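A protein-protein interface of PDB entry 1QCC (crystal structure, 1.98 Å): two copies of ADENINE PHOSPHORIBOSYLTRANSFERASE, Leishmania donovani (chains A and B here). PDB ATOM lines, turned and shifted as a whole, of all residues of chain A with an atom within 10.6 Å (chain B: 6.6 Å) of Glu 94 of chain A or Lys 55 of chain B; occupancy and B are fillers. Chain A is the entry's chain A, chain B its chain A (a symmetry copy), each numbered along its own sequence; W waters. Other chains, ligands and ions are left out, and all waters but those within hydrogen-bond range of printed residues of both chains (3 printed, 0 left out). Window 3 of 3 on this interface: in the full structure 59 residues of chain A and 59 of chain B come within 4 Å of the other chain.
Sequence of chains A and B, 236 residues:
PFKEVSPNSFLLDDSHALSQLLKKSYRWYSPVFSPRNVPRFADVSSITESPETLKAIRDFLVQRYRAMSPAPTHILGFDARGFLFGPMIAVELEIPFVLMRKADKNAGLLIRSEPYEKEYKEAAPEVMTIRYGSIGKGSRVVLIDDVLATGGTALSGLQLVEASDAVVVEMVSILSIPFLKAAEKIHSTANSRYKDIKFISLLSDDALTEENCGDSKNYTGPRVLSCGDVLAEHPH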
ATOM      1  N   ARG A  58      18.252  17.151  26.357  1.00  0.00           N
ATOM      2  CA  ARG A  58      19.041  18.377  26.302  1.00  0.00           C
ATOM      3  C   ARG A  58      18.627  19.352  27.409  1.00  0.00           C
ATOM      4  O   ARG A  58      19.470  19.851  28.149  1.00  0.00           O
ATOM      5  CB  ARG A  58      18.867  19.028  24.919  1.00  0.00           C
ATOM      6  CG  ARG A  58      19.837  20.157  24.577  1.00  0.00           C
ATOM      7  CD  ARG A  58      19.444  21.497  25.200  1.00  0.00           C
ATOM      8  NE  ARG A  58      18.070  21.891  24.884  1.00  0.00           N
ATOM      9  CZ  ARG A  58      17.674  22.438  23.735  1.00  0.00           C
ATOM     10  NH1 ARG A  58      16.399  22.755  23.565  1.00  0.00           N
ATOM     11  NH2 ARG A  58      18.541  22.665  22.753  1.00  0.00           N
ATOM     12  N   LEU A  61      19.414  17.865  31.214  1.00  0.00           N
ATOM     13  CA  LEU A  61      20.835  17.889  31.545  1.00  0.00           C
ATOM     14  C   LEU A  61      21.447  19.289  31.586  1.00  0.00           C
ATOM     15  O   LEU A  61      22.271  19.577  32.461  1.00  0.00           O
ATOM     16  CB  LEU A  61      21.622  16.945  30.633  1.00  0.00           C
ATOM     17  CG  LEU A  61      21.307  15.461  30.891  1.00  0.00           C
ATOM     18  CD1 LEU A  61      22.045  14.549  29.918  1.00  0.00           C
ATOM     19  CD2 LEU A  61      21.673  15.107  32.327  1.00  0.00           C
ATOM     20  N   VAL A  62      21.037  20.164  30.668  1.00  0.00           N
ATOM     21  CA  VAL A  62      21.543  21.539  30.656  1.00  0.00           C
ATOM     22  C   VAL A  62      21.108  22.233  31.949  1.00  0.00           C
ATOM     23  O   VAL A  62      21.915  22.892  32.604  1.00  0.00           O
ATOM     24  CB  VAL A  62      21.035  22.340  29.436  1.00  0.00           C
ATOM     25  CG1 VAL A  62      21.274  23.822  29.646  1.00  0.00           C
ATOM     26  CG2 VAL A  62      21.759  21.893  28.188  1.00  0.00           C
ATOM     27  N   TYR A  65      23.208  20.953  34.889  1.00  0.00           N
ATOM     28  CA  TYR A  65      24.559  21.485  35.003  1.00  0.00           C
ATOM     29  C   TYR A  65      24.644  22.990  35.245  1.00  0.00           C
ATOM     30  O   TYR A  65      25.645  23.475  35.776  1.00  0.00           O
ATOM     31  CB  TYR A  65      25.425  21.012  33.831  1.00  0.00           C
ATOM     32  CG  TYR A  65      25.529  19.496  33.783  1.00  0.00           C
ATOM     33  CD1 TYR A  65      25.919  18.767  34.914  1.00  0.00           C
ATOM     34  CD2 TYR A  65      25.157  18.785  32.642  1.00  0.00           C
ATOM     35  CE1 TYR A  65      25.925  17.371  34.913  1.00  0.00           C
ATOM     36  CE2 TYR A  65      25.158  17.387  32.629  1.00  0.00           C
ATOM     37  CZ  TYR A  65      25.538  16.690  33.766  1.00  0.00           C
ATOM     38  OH  TYR A  65      25.504  15.316  33.756  1.00  0.00           O
ATOM     39  N   ARG A  66      23.583  23.719  34.895  1.00  0.00           N
ATOM     40  CA  ARG A  66      23.527  25.167  35.135  1.00  0.00           C
ATOM     41  C   ARG A  66      23.275  25.429  36.623  1.00  0.00           C
ATOM     42  O   ARG A  66      23.768  26.412  37.187  1.00  0.00           O
ATOM     43  CB  ARG A  66      22.426  25.827  34.304  1.00  0.00           C
ATOM     44  CG  ARG A  66      22.846  26.140  32.889  1.00  0.00           C
ATOM     45  CD  ARG A  66      21.814  26.980  32.159  1.00  0.00           C
ATOM     46  NE  ARG A  66      22.277  27.307  30.813  1.00  0.00           N
ATOM     47  CZ  ARG A  66      21.494  27.359  29.743  1.00  0.00           C
ATOM     48  NH1 ARG A  66      20.198  27.114  29.861  1.00  0.00           N
ATOM     49  NH2 ARG A  66      22.009  27.612  28.547  1.00  0.00           N
ATOM     50  N   ALA A  71      30.178  24.321  38.922  1.00  0.00           N
ATOM     51  CA  ALA A  71      29.758  23.926  37.580  1.00  0.00           C
ATOM     52  C   ALA A  71      30.830  23.155  36.800  1.00  0.00           C
ATOM     53  O   ALA A  71      32.032  23.398  36.962  1.00  0.00           O
ATOM     54  CB  ALA A  71      29.321  25.151  36.794  1.00  0.00           C
ATOM     55  N   PRO A  72      30.404  22.192  35.963  1.00  0.00           N
ATOM     56  CA  PRO A  72      31.335  21.391  35.160  1.00  0.00           C
ATOM     57  C   PRO A  72      32.120  22.298  34.214  1.00  0.00           C
ATOM     58  O   PRO A  72      31.623  23.339  33.788  1.00  0.00           O
ATOM     59  CB  PRO A  72      30.401  20.472  34.377  1.00  0.00           C
ATOM     60  CG  PRO A  72      29.215  20.332  35.287  1.00  0.00           C
ATOM     61  CD  PRO A  72      29.017  21.736  35.765  1.00  0.00           C
ATOM     62  N   THR A  73      33.352  21.916  33.903  1.00  0.00           N
ATOM     63  CA  THR A  73      34.178  22.709  33.003  1.00  0.00           C
ATOM     64  C   THR A  73      34.262  22.050  31.631  1.00  0.00           C
ATOM     65  O   THR A  73      34.503  22.722  30.630  1.00  0.00           O
ATOM     66  CB  THR A  73      35.604  22.894  33.565  1.00  0.00           C
ATOM     67  OG1 THR A  73      36.237  21.617  33.688  1.00  0.00           O
ATOM     68  CG2 THR A  73      35.558  23.552  34.935  1.00  0.00           C
ATOM     69  N   HIS A  74      34.048  20.735  31.592  1.00  0.00           N
ATOM     70  CA  HIS A  74      34.113  19.965  30.349  1.00  0.00           C
ATOM     71  C   HIS A  74      33.091  18.833  30.313  1.00  0.00           C
ATOM     72  O   HIS A  74      32.629  18.344  31.348  1.00  0.00           O
ATOM     73  CB  HIS A  74      35.487  19.281  30.179  1.00  0.00           C
ATOM     74  CG  HIS A  74      36.653  20.215  30.067  1.00  0.00           C
ATOM     75  ND1 HIS A  74      37.232  20.823  31.159  1.00  0.00           N
ATOM     76  CD2 HIS A  74      37.398  20.583  28.996  1.00  0.00           C
ATOM     77  CE1 HIS A  74      38.282  21.523  30.769  1.00  0.00           C
ATOM     78  NE2 HIS A  74      38.406  21.393  29.460  1.00  0.00           N
ATOM     79  N   ILE A  75      32.798  18.391  29.095  1.00  0.00           N
ATOM     80  CA  ILE A  75      31.913  17.263  28.839  1.00  0.00           C
ATOM     81  C   ILE A  75      32.767  16.312  27.973  1.00  0.00           C
ATOM     82  O   ILE A  75      33.309  16.719  26.939  1.00  0.00           O
ATOM     83  CB  ILE A  75      30.655  17.668  28.038  1.00  0.00           C
ATOM     84  CG1 ILE A  75      29.805  18.698  28.804  1.00  0.00           C
ATOM     85  CG2 ILE A  75      29.846  16.425  27.682  1.00  0.00           C
ATOM     86  CD1 ILE A  75      29.163  18.184  30.056  1.00  0.00           C
ATOM     87  N   GLY A  86      26.467  14.781  23.902  1.00  0.00           N
ATOM     88  CA  GLY A  86      27.382  15.735  24.507  1.00  0.00           C
ATOM     89  C   GLY A  86      27.403  17.150  23.959  1.00  0.00           C
ATOM     90  O   GLY A  86      27.209  18.103  24.719  1.00  0.00           O
ATOM     91  N   PRO A  87      27.658  17.322  22.649  1.00  0.00           N
ATOM     92  CA  PRO A  87      27.711  18.636  21.993  1.00  0.00           C
ATOM     93  C   PRO A  87      26.496  19.547  22.197  1.00  0.00           C
ATOM     94  O   PRO A  87      26.663  20.752  22.373  1.00  0.00           O
ATOM     95  CB  PRO A  87      27.899  18.268  20.521  1.00  0.00           C
ATOM     96  CG  PRO A  87      28.717  17.007  20.599  1.00  0.00           C
ATOM     97  CD  PRO A  87      28.008  16.251  21.699  1.00  0.00           C
ATOM     98  N   MET A  88      25.282  18.989  22.178  1.00  0.00           N
ATOM     99  CA  MET A  88      24.091  19.817  22.357  1.00  0.00           C
ATOM    100  C   MET A  88      23.952  20.335  23.788  1.00  0.00           C
ATOM    101  O   MET A  88      23.253  21.318  24.033  1.00  0.00           O
ATOM    102  CB  MET A  88      22.820  19.099  21.891  1.00  0.00           C
ATOM    103  CG  MET A  88      22.318  18.005  22.798  1.00  0.00           C
ATOM    104  SD  MET A  88      20.829  17.211  22.145  1.00  0.00           S
ATOM    105  CE  MET A  88      20.709  15.860  23.317  1.00  0.00           C
ATOM    106  N   ILE A  89      24.630  19.683  24.727  1.00  0.00           N
ATOM    107  CA  ILE A  89      24.604  20.127  26.115  1.00  0.00           C
ATOM    108  C   ILE A  89      25.743  21.129  26.302  1.00  0.00           C
ATOM    109  O   ILE A  89      25.548  22.207  26.864  1.00  0.00           O
ATOM    110  CB  ILE A  89      24.793  18.948  27.093  1.00  0.00           C
ATOM    111  CG1 ILE A  89      23.656  17.937  26.932  1.00  0.00           C
ATOM    112  CG2 ILE A  89      24.837  19.454  28.534  1.00  0.00           C
ATOM    113  CD1 ILE A  89      23.872  16.665  27.719  1.00  0.00           C
ATOM    114  N   ALA A  90      26.919  20.775  25.786  1.00  0.00           N
ATOM    115  CA  ALA A  90      28.106  21.619  25.886  1.00  0.00           C
ATOM    116  C   ALA A  90      27.934  22.982  25.220  1.00  0.00           C
ATOM    117  O   ALA A  90      28.437  23.983  25.722  1.00  0.00           O
ATOM    118  CB  ALA A  90      29.333  20.891  25.313  1.00  0.00           C
ATOM    119  N   VAL A  91      27.213  23.020  24.103  1.00  0.00           N
ATOM    120  CA  VAL A  91      26.983  24.270  23.377  1.00  0.00           C
ATOM    121  C   VAL A  91      26.151  25.259  24.210  1.00  0.00           C
ATOM    122  O   VAL A  91      26.381  26.467  24.170  1.00  0.00           O
ATOM    123  CB  VAL A  91      26.328  24.013  21.979  1.00  0.00           C
ATOM    124  CG1 VAL A  91      24.890  23.554  22.119  1.00  0.00           C
ATOM    125  CG2 VAL A  91      26.410  25.251  21.122  1.00  0.00           C
ATOM    126  N   GLU A  92      25.229  24.731  25.009  1.00  0.00           N
ATOM    127  CA  GLU A  92      24.388  25.561  25.863  1.00  0.00           C
ATOM    128  C   GLU A  92      25.136  26.014  27.118  1.00  0.00           C
ATOM    129  O   GLU A  92      24.971  27.144  27.576  1.00  0.00           O
ATOM    130  CB  GLU A  92      23.126  24.799  26.263  1.00  0.00           C
ATOM    131  CG  GLU A  92      22.230  24.426  25.098  1.00  0.00           C
ATOM    132  CD  GLU A  92      21.719  25.633  24.324  1.00  0.00           C
ATOM    133  OE1 GLU A  92      21.519  26.710  24.927  1.00  0.00           O
ATOM    134  OE2 GLU A  92      21.507  25.500  23.105  1.00  0.00           O
ATOM    135  N   LEU A  93      25.929  25.114  27.691  1.00  0.00           N
ATOM    136  CA  LEU A  93      26.712  25.418  28.882  1.00  0.00           C
ATOM    137  C   LEU A  93      27.919  26.262  28.514  1.00  0.00           C
ATOM    138  O   LEU A  93      28.581  26.818  29.386  1.00  0.00           O
ATOM    139  CB  LEU A  93      27.204  24.129  29.541  1.00  0.00           C
ATOM    140  CG  LEU A  93      26.148  23.171  30.085  1.00  0.00           C
ATOM    141  CD1 LEU A  93      26.835  21.935  30.623  1.00  0.00           C
ATOM    142  CD2 LEU A  93      25.331  23.850  31.162  1.00  0.00           C
ATOM    143  N   GLU A  94      28.223  26.316  27.218  1.00  0.00           N
ATOM    144  CA  GLU A  94      29.359  27.072  26.702  1.00  0.00           C
ATOM    145  C   GLU A  94      30.685  26.544  27.230  1.00  0.00           C
ATOM    146  O   GLU A  94      31.544  27.312  27.659  1.00  0.00           O
ATOM    147  CB  GLU A  94      29.203  28.565  27.009  1.00  0.00           C
ATOM    148  CG  GLU A  94      27.988  29.180  26.329  1.00  0.00           C
ATOM    149  CD  GLU A  94      27.795  30.661  26.634  1.00  0.00           C
ATOM    150  OE1 GLU A  94      26.963  31.286  25.940  1.00  0.00           O
ATOM    151  OE2 GLU A  94      28.456  31.193  27.559  1.00  0.00           O
ATOM    152  N   ILE A  95      30.818  25.221  27.252  1.00  0.00           N
ATOM    153  CA  ILE A  95      32.052  24.581  27.695  1.00  0.00           C
ATOM    154  C   ILE A  95      32.515  23.629  26.601  1.00  0.00           C
ATOM    155  O   ILE A  95      31.752  23.284  25.696  1.00  0.00           O
ATOM    156  CB  ILE A  95      31.894  23.814  29.043  1.00  0.00           C
ATOM    157  CG1 ILE A  95      30.761  22.786  28.957  1.00  0.00           C
ATOM    158  CG2 ILE A  95      31.695  24.798  30.196  1.00  0.00           C
ATOM    159  CD1 ILE A  95      30.622  21.934  30.204  1.00  0.00           C
ATOM    160  N   PRO A  96      33.792  23.224  26.645  1.00  0.00           N
ATOM    161  CA  PRO A  96      34.362  22.313  25.653  1.00  0.00           C
ATOM    162  C   PRO A  96      33.782  20.901  25.673  1.00  0.00           C
ATOM    163  O   PRO A  96      33.418  20.383  26.737  1.00  0.00           O
ATOM    164  CB  PRO A  96      35.836  22.261  26.061  1.00  0.00           C
ATOM    165  CG  PRO A  96      36.064  23.572  26.720  1.00  0.00           C
ATOM    166  CD  PRO A  96      34.836  23.722  27.553  1.00  0.00           C
ATOM    167  N   PHE A  97      33.649  20.310  24.485  1.00  0.00           N
ATOM    168  CA  PHE A  97      33.215  18.927  24.367  1.00  0.00           C
ATOM    169  C   PHE A  97      34.473  18.185  23.916  1.00  0.00           C
ATOM    170  O   PHE A  97      35.005  18.449  22.838  1.00  0.00           O
ATOM    171  CB  PHE A  97      32.098  18.715  23.334  1.00  0.00           C
ATOM    172  CG  PHE A  97      31.741  17.257  23.144  1.00  0.00           C
ATOM    173  CD1 PHE A  97      31.046  16.563  24.133  1.00  0.00           C
ATOM    174  CD2 PHE A  97      32.181  16.552  22.022  1.00  0.00           C
ATOM    175  CE1 PHE A  97      30.802  15.194  24.017  1.00  0.00           C
ATOM    176  CE2 PHE A  97      31.942  15.177  21.895  1.00  0.00           C
ATOM    177  CZ  PHE A  97      31.253  14.500  22.894  1.00  0.00           C
ATOM    178  N   VAL A  98      34.968  17.294  24.767  1.00  0.00           N
ATOM    179  CA  VAL A  98      36.170  16.517  24.472  1.00  0.00           C
ATOM    180  C   VAL A  98      35.776  15.116  23.993  1.00  0.00           C
ATOM    181  O   VAL A  98      34.772  14.550  24.434  1.00  0.00           O
ATOM    182  CB  VAL A  98      37.108  16.453  25.714  1.00  0.00           C
ATOM    183  CG1 VAL A  98      38.399  15.700  25.388  1.00  0.00           C
ATOM    184  CG2 VAL A  98      37.426  17.870  26.195  1.00  0.00           C
ATOM    185  N   SER B  50      35.774  24.255  21.254  1.00  0.00           N
ATOM    186  CA  SER B  50      35.622  25.708  21.180  1.00  0.00           C
ATOM    187  C   SER B  50      34.126  26.039  21.292  1.00  0.00           C
ATOM    188  O   SER B  50      33.381  25.940  20.313  1.00  0.00           O
ATOM    189  CB  SER B  50      36.194  26.243  19.861  1.00  0.00           C
ATOM    190  OG  SER B  50      35.914  27.626  19.708  1.00  0.00           O
ATOM    191  N   PRO B  51      33.669  26.428  22.497  1.00  0.00           N
ATOM    192  CA  PRO B  51      32.268  26.769  22.761  1.00  0.00           C
ATOM    193  C   PRO B  51      31.699  27.800  21.799  1.00  0.00           C
ATOM    194  O   PRO B  51      30.600  27.624  21.268  1.00  0.00           O
ATOM    195  CB  PRO B  51      32.320  27.312  24.182  1.00  0.00           C
ATOM    196  CG  PRO B  51      33.424  26.534  24.787  1.00  0.00           C
ATOM    197  CD  PRO B  51      34.475  26.569  23.720  1.00  0.00           C
ATOM    198  N   GLU B  52      32.458  28.866  21.568  1.00  0.00           N
ATOM    199  CA  GLU B  52      32.032  29.941  20.671  1.00  0.00           C
ATOM    200  C   GLU B  52      31.880  29.449  19.229  1.00  0.00           C
ATOM    201  O   GLU B  52      30.901  29.775  18.550  1.00  0.00           O
ATOM    202  CB  GLU B  52      33.029  31.105  20.740  1.00  0.00           C
ATOM    203  CG  GLU B  52      32.561  32.386  20.056  1.00  0.00           C
ATOM    204  CD  GLU B  52      33.633  33.479  20.008  1.00  0.00           C
ATOM    205  OE1 GLU B  52      34.810  33.198  20.336  1.00  0.00           O
ATOM    206  OE2 GLU B  52      33.295  34.622  19.625  1.00  0.00           O
ATOM    207  N   THR B  53      32.834  28.643  18.772  1.00  0.00           N
ATOM    208  CA  THR B  53      32.783  28.123  17.412  1.00  0.00           C
ATOM    209  C   THR B  53      31.642  27.122  17.244  1.00  0.00           C
ATOM    210  O   THR B  53      30.925  27.159  16.241  1.00  0.00           O
ATOM    211  CB  THR B  53      34.119  27.478  16.996  1.00  0.00           C
ATOM    212  OG1 THR B  53      35.194  28.369  17.305  1.00  0.00           O
ATOM    213  CG2 THR B  53      34.134  27.210  15.500  1.00  0.00           C
ATOM    214  N   LEU B  54      31.453  26.255  18.239  1.00  0.00           N
ATOM    215  CA  LEU B  54      30.381  25.260  18.191  1.00  0.00           C
ATOM    216  C   LEU B  54      29.013  25.952  18.130  1.00  0.00           C
ATOM    217  O   LEU B  54      28.146  25.574  17.339  1.00  0.00           O
ATOM    218  CB  LEU B  54      30.455  24.333  19.410  1.00  0.00           C
ATOM    219  CG  LEU B  54      29.628  23.049  19.321  1.00  0.00           C
ATOM    220  CD1 LEU B  54      30.082  22.212  18.116  1.00  0.00           C
ATOM    221  CD2 LEU B  54      29.779  22.257  20.603  1.00  0.00           C
ATOM    222  N   LYS B  55      28.840  26.984  18.948  1.00  0.00           N
ATOM    223  CA  LYS B  55      27.594  27.741  18.986  1.00  0.00           C
ATOM    224  C   LYS B  55      27.341  28.485  17.666  1.00  0.00           C
ATOM    225  O   LYS B  55      26.204  28.567  17.197  1.00  0.00           O
ATOM    226  CB  LYS B  55      27.614  28.724  20.159  1.00  0.00           C
ATOM    227  CG  LYS B  55      26.292  29.447  20.377  1.00  0.00           C
ATOM    228  CD  LYS B  55      26.328  30.315  21.612  1.00  0.00           C
ATOM    229  CE  LYS B  55      25.006  31.022  21.811  1.00  0.00           C
ATOM    230  NZ  LYS B  55      24.965  31.745  23.115  1.00  0.00           N
ATOM    231  N   ALA B  56      28.407  29.012  17.065  1.00  0.00           N
ATOM    232  CA  ALA B  56      28.293  29.737  15.801  1.00  0.00           C
ATOM    233  C   ALA B  56      27.827  28.806  14.677  1.00  0.00           C
ATOM    234  O   ALA B  56      27.037  29.200  13.814  1.00  0.00           O
ATOM    235  CB  ALA B  56      29.625  30.396  15.442  1.00  0.00           C
ATOM    236  N   ILE B  57      28.315  27.569  14.697  1.00  0.00           N
ATOM    237  CA  ILE B  57      27.927  26.574  13.702  1.00  0.00           C
ATOM    238  C   ILE B  57      26.438  26.228  13.878  1.00  0.00           C
ATOM    239  O   ILE B  57      25.675  26.195  12.911  1.00  0.00           O
ATOM    240  CB  ILE B  57      28.781  25.292  13.848  1.00  0.00           C
ATOM    241  CG1 ILE B  57      30.234  25.590  13.473  1.00  0.00           C
ATOM    242  CG2 ILE B  57      28.194  24.153  13.006  1.00  0.00           C
ATOM    243  CD1 ILE B  57      31.185  24.455  13.757  1.00  0.00           C
ATOM    244  N   ARG B  58      26.042  25.989  15.126  1.00  0.00           N
ATOM    245  CA  ARG B  58      24.665  25.653  15.474  1.00  0.00           C
ATOM    246  C   ARG B  58      23.700  26.768  15.056  1.00  0.00           C
ATOM    247  O   ARG B  58      22.698  26.512  14.396  1.00  0.00           O
ATOM    248  CB  ARG B  58      24.574  25.405  16.990  1.00  0.00           C
ATOM    249  CG  ARG B  58      23.282  24.764  17.493  1.00  0.00           C
ATOM    250  CD  ARG B  58      22.133  25.761  17.640  1.00  0.00           C
ATOM    251  NE  ARG B  58      22.486  26.917  18.467  1.00  0.00           N
ATOM    252  CZ  ARG B  58      22.514  26.927  19.799  1.00  0.00           C
ATOM    253  NH1 ARG B  58      22.848  28.037  20.439  1.00  0.00           N
ATOM    254  NH2 ARG B  58      22.219  25.834  20.496  1.00  0.00           N
ATOM    255  N   ASP B  59      24.019  28.005  15.430  1.00  0.00           N
ATOM    256  CA  ASP B  59      23.174  29.153  15.115  1.00  0.00           C
ATOM    257  C   ASP B  59      23.014  29.387  13.628  1.00  0.00           C
ATOM    258  O   ASP B  59      21.903  29.581  13.150  1.00  0.00           O
ATOM    259  CB  ASP B  59      23.713  30.432  15.763  1.00  0.00           C
ATOM    260  CG  ASP B  59      23.632  30.412  17.279  1.00  0.00           C
ATOM    261  OD1 ASP B  59      24.374  31.191  17.909  1.00  0.00           O
ATOM    262  OD2 ASP B  59      22.829  29.643  17.847  1.00  0.00           O
ATOM    263  N   PHE B  60      24.128  29.374  12.901  1.00  0.00           N
ATOM    264  CA  PHE B  60      24.105  29.599  11.464  1.00  0.00           C
ATOM    265  C   PHE B  60      23.258  28.562  10.722  1.00  0.00           C
ATOM    266  O   PHE B  60      22.333  28.919   9.988  1.00  0.00           O
ATOM    267  CB  PHE B  60      25.533  29.622  10.907  1.00  0.00           C
ATOM    268  CG  PHE B  60      25.604  29.915   9.431  1.00  0.00           C
ATOM    269  CD1 PHE B  60      25.687  31.224   8.973  1.00  0.00           C
ATOM    270  CD2 PHE B  60      25.568  28.880   8.498  1.00  0.00           C
ATOM    271  CE1 PHE B  60      25.730  31.504   7.609  1.00  0.00           C
ATOM    272  CE2 PHE B  60      25.610  29.149   7.130  1.00  0.00           C
ATOM    273  CZ  PHE B  60      25.692  30.469   6.688  1.00  0.00           C
ATOM    274  N   MET B  88      22.579  18.741  17.522  1.00  0.00           N
ATOM    275  CA  MET B  88      22.342  20.080  18.057  1.00  0.00           C
ATOM    276  C   MET B  88      21.557  20.963  17.088  1.00  0.00           C
ATOM    277  O   MET B  88      20.952  21.956  17.494  1.00  0.00           O
ATOM    278  CB  MET B  88      23.640  20.755  18.509  1.00  0.00           C
ATOM    279  CG  MET B  88      24.539  21.248  17.404  1.00  0.00           C
ATOM    280  SD  MET B  88      26.051  22.006  18.045  1.00  0.00           S
ATOM    281  CE  MET B  88      26.929  22.210  16.495  1.00  0.00           C
HETATM  282  O   HOH W   1      24.643  29.351  25.622  1.00  0.00           O
HETATM  283  O   HOH W   2      28.662  27.593  23.342  1.00  0.00           O
HETATM  284  O   HOH W   3      22.759  28.702  23.322  1.00  0.00           O
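The guanidinium group of Arg 58 of chain B lies within salt-bridge range of the side-chain carboxylate of Glu 92 of chain A (2.7 Å).
The side-chain carboxylate of Glu 94 of chain A is in salt-bridge range of the side-chain amino group of Lys 55 of chain B, 3.5 Å away.
NH2 of Arg 66 of chain A is in salt-bridge range of OE1 of Glu 92 of chain A (3.8 Å).
N of Ile 75 of chain A sits at hydrogen-bond distance from O of Pro 96 of chain A.
The backbone carbonyl oxygen (O) of Ala 90 of chain A sits at hydrogen-bond distance from the backbone NH (N) of Ile 95 of chain A.
NE of Arg 58 of chain B lies within salt-bridge range of OD2 of Asp 59 of chain B (2.8 Å).
Among the printed residues, merely in contact across the chains: Val 91 of chain A with Lys 55 of chain B (3.5 Å), Glu 94 of chain A with Pro 51 of chain B (3.5 Å), Ile 95 of chain A with Pro 51 of chain B (3.5 Å), Pro 96 of chain A with Pro 51 of chain B (3.8 Å), Met 88 of chain A with Met 88 of chain B (3.9 Å), Val 91 of chain A with Arg 58 of chain B (3.9 Å) and Pro 87 of chain A with Leu 54 of chain B (3.9 Å).
Glu 94 of chain A touches two residues of chain B.
Of chain A, only Val 91 (3.5 Å) and Glu 94 (3.5 Å) come within 4 Å of Lys 55 of chain B.
Of chain A, only Glu 94, Ile 95 and Pro 96 come within 4 Å of Pro 51 of chain B.
No residue of chain A comes within 4 Å of Ala 56 of chain B.
Of chain A, only Val 91 (3.9 Å) and Glu 92 (2.7 Å) come within 4 Å of Arg 58 of chain B.
Printed residues of chain B within 4 Å of Pro 96 of chain A: Pro 51 (3.8 Å).
Of the printed residues of chain B, Pro 87 of chain A touches Leu 54.
Of the printed residues of chain B, Glu 92 of chain A touches Arg 58 (2.7 Å).
The nearest residue of chain A that does not touch Lys 55 of chain B is Glu 92 of chain A (6.4 Å).
Of the 12 printed residues of chain B, 5 touch a printed residue of chain A.
Among the printed residues, 9 pairs touch across the chains.
Among the printed residues, Asp or Glu carboxylates within 4 Å of a Lys or Arg side-chain nitrogen of the other chain: Glu 92 of chain A with Arg 58 of chain B (2.7 Å) and Glu 94 of chain A with Lys 55 of chain B (3.5 Å).
Met 88 of chain B touches its own counterpart, Met 88 of chain A.
Water W2 bridges O of Val 91 of chain A (2.7 Å) and O of Pro 51 of chain B (2.8 Å).
Water W3 bridges the side-chain carboxylate of Glu 92 of chain A (2.8 Å) and the guanidinium group of Arg 58 of chain B (3.0 Å).
Water W1 lies within hydrogen-bond range of O of Glu 92 of chain A, OE1 of Glu 94 of chain A and NZ of Lys 55 of chain B.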
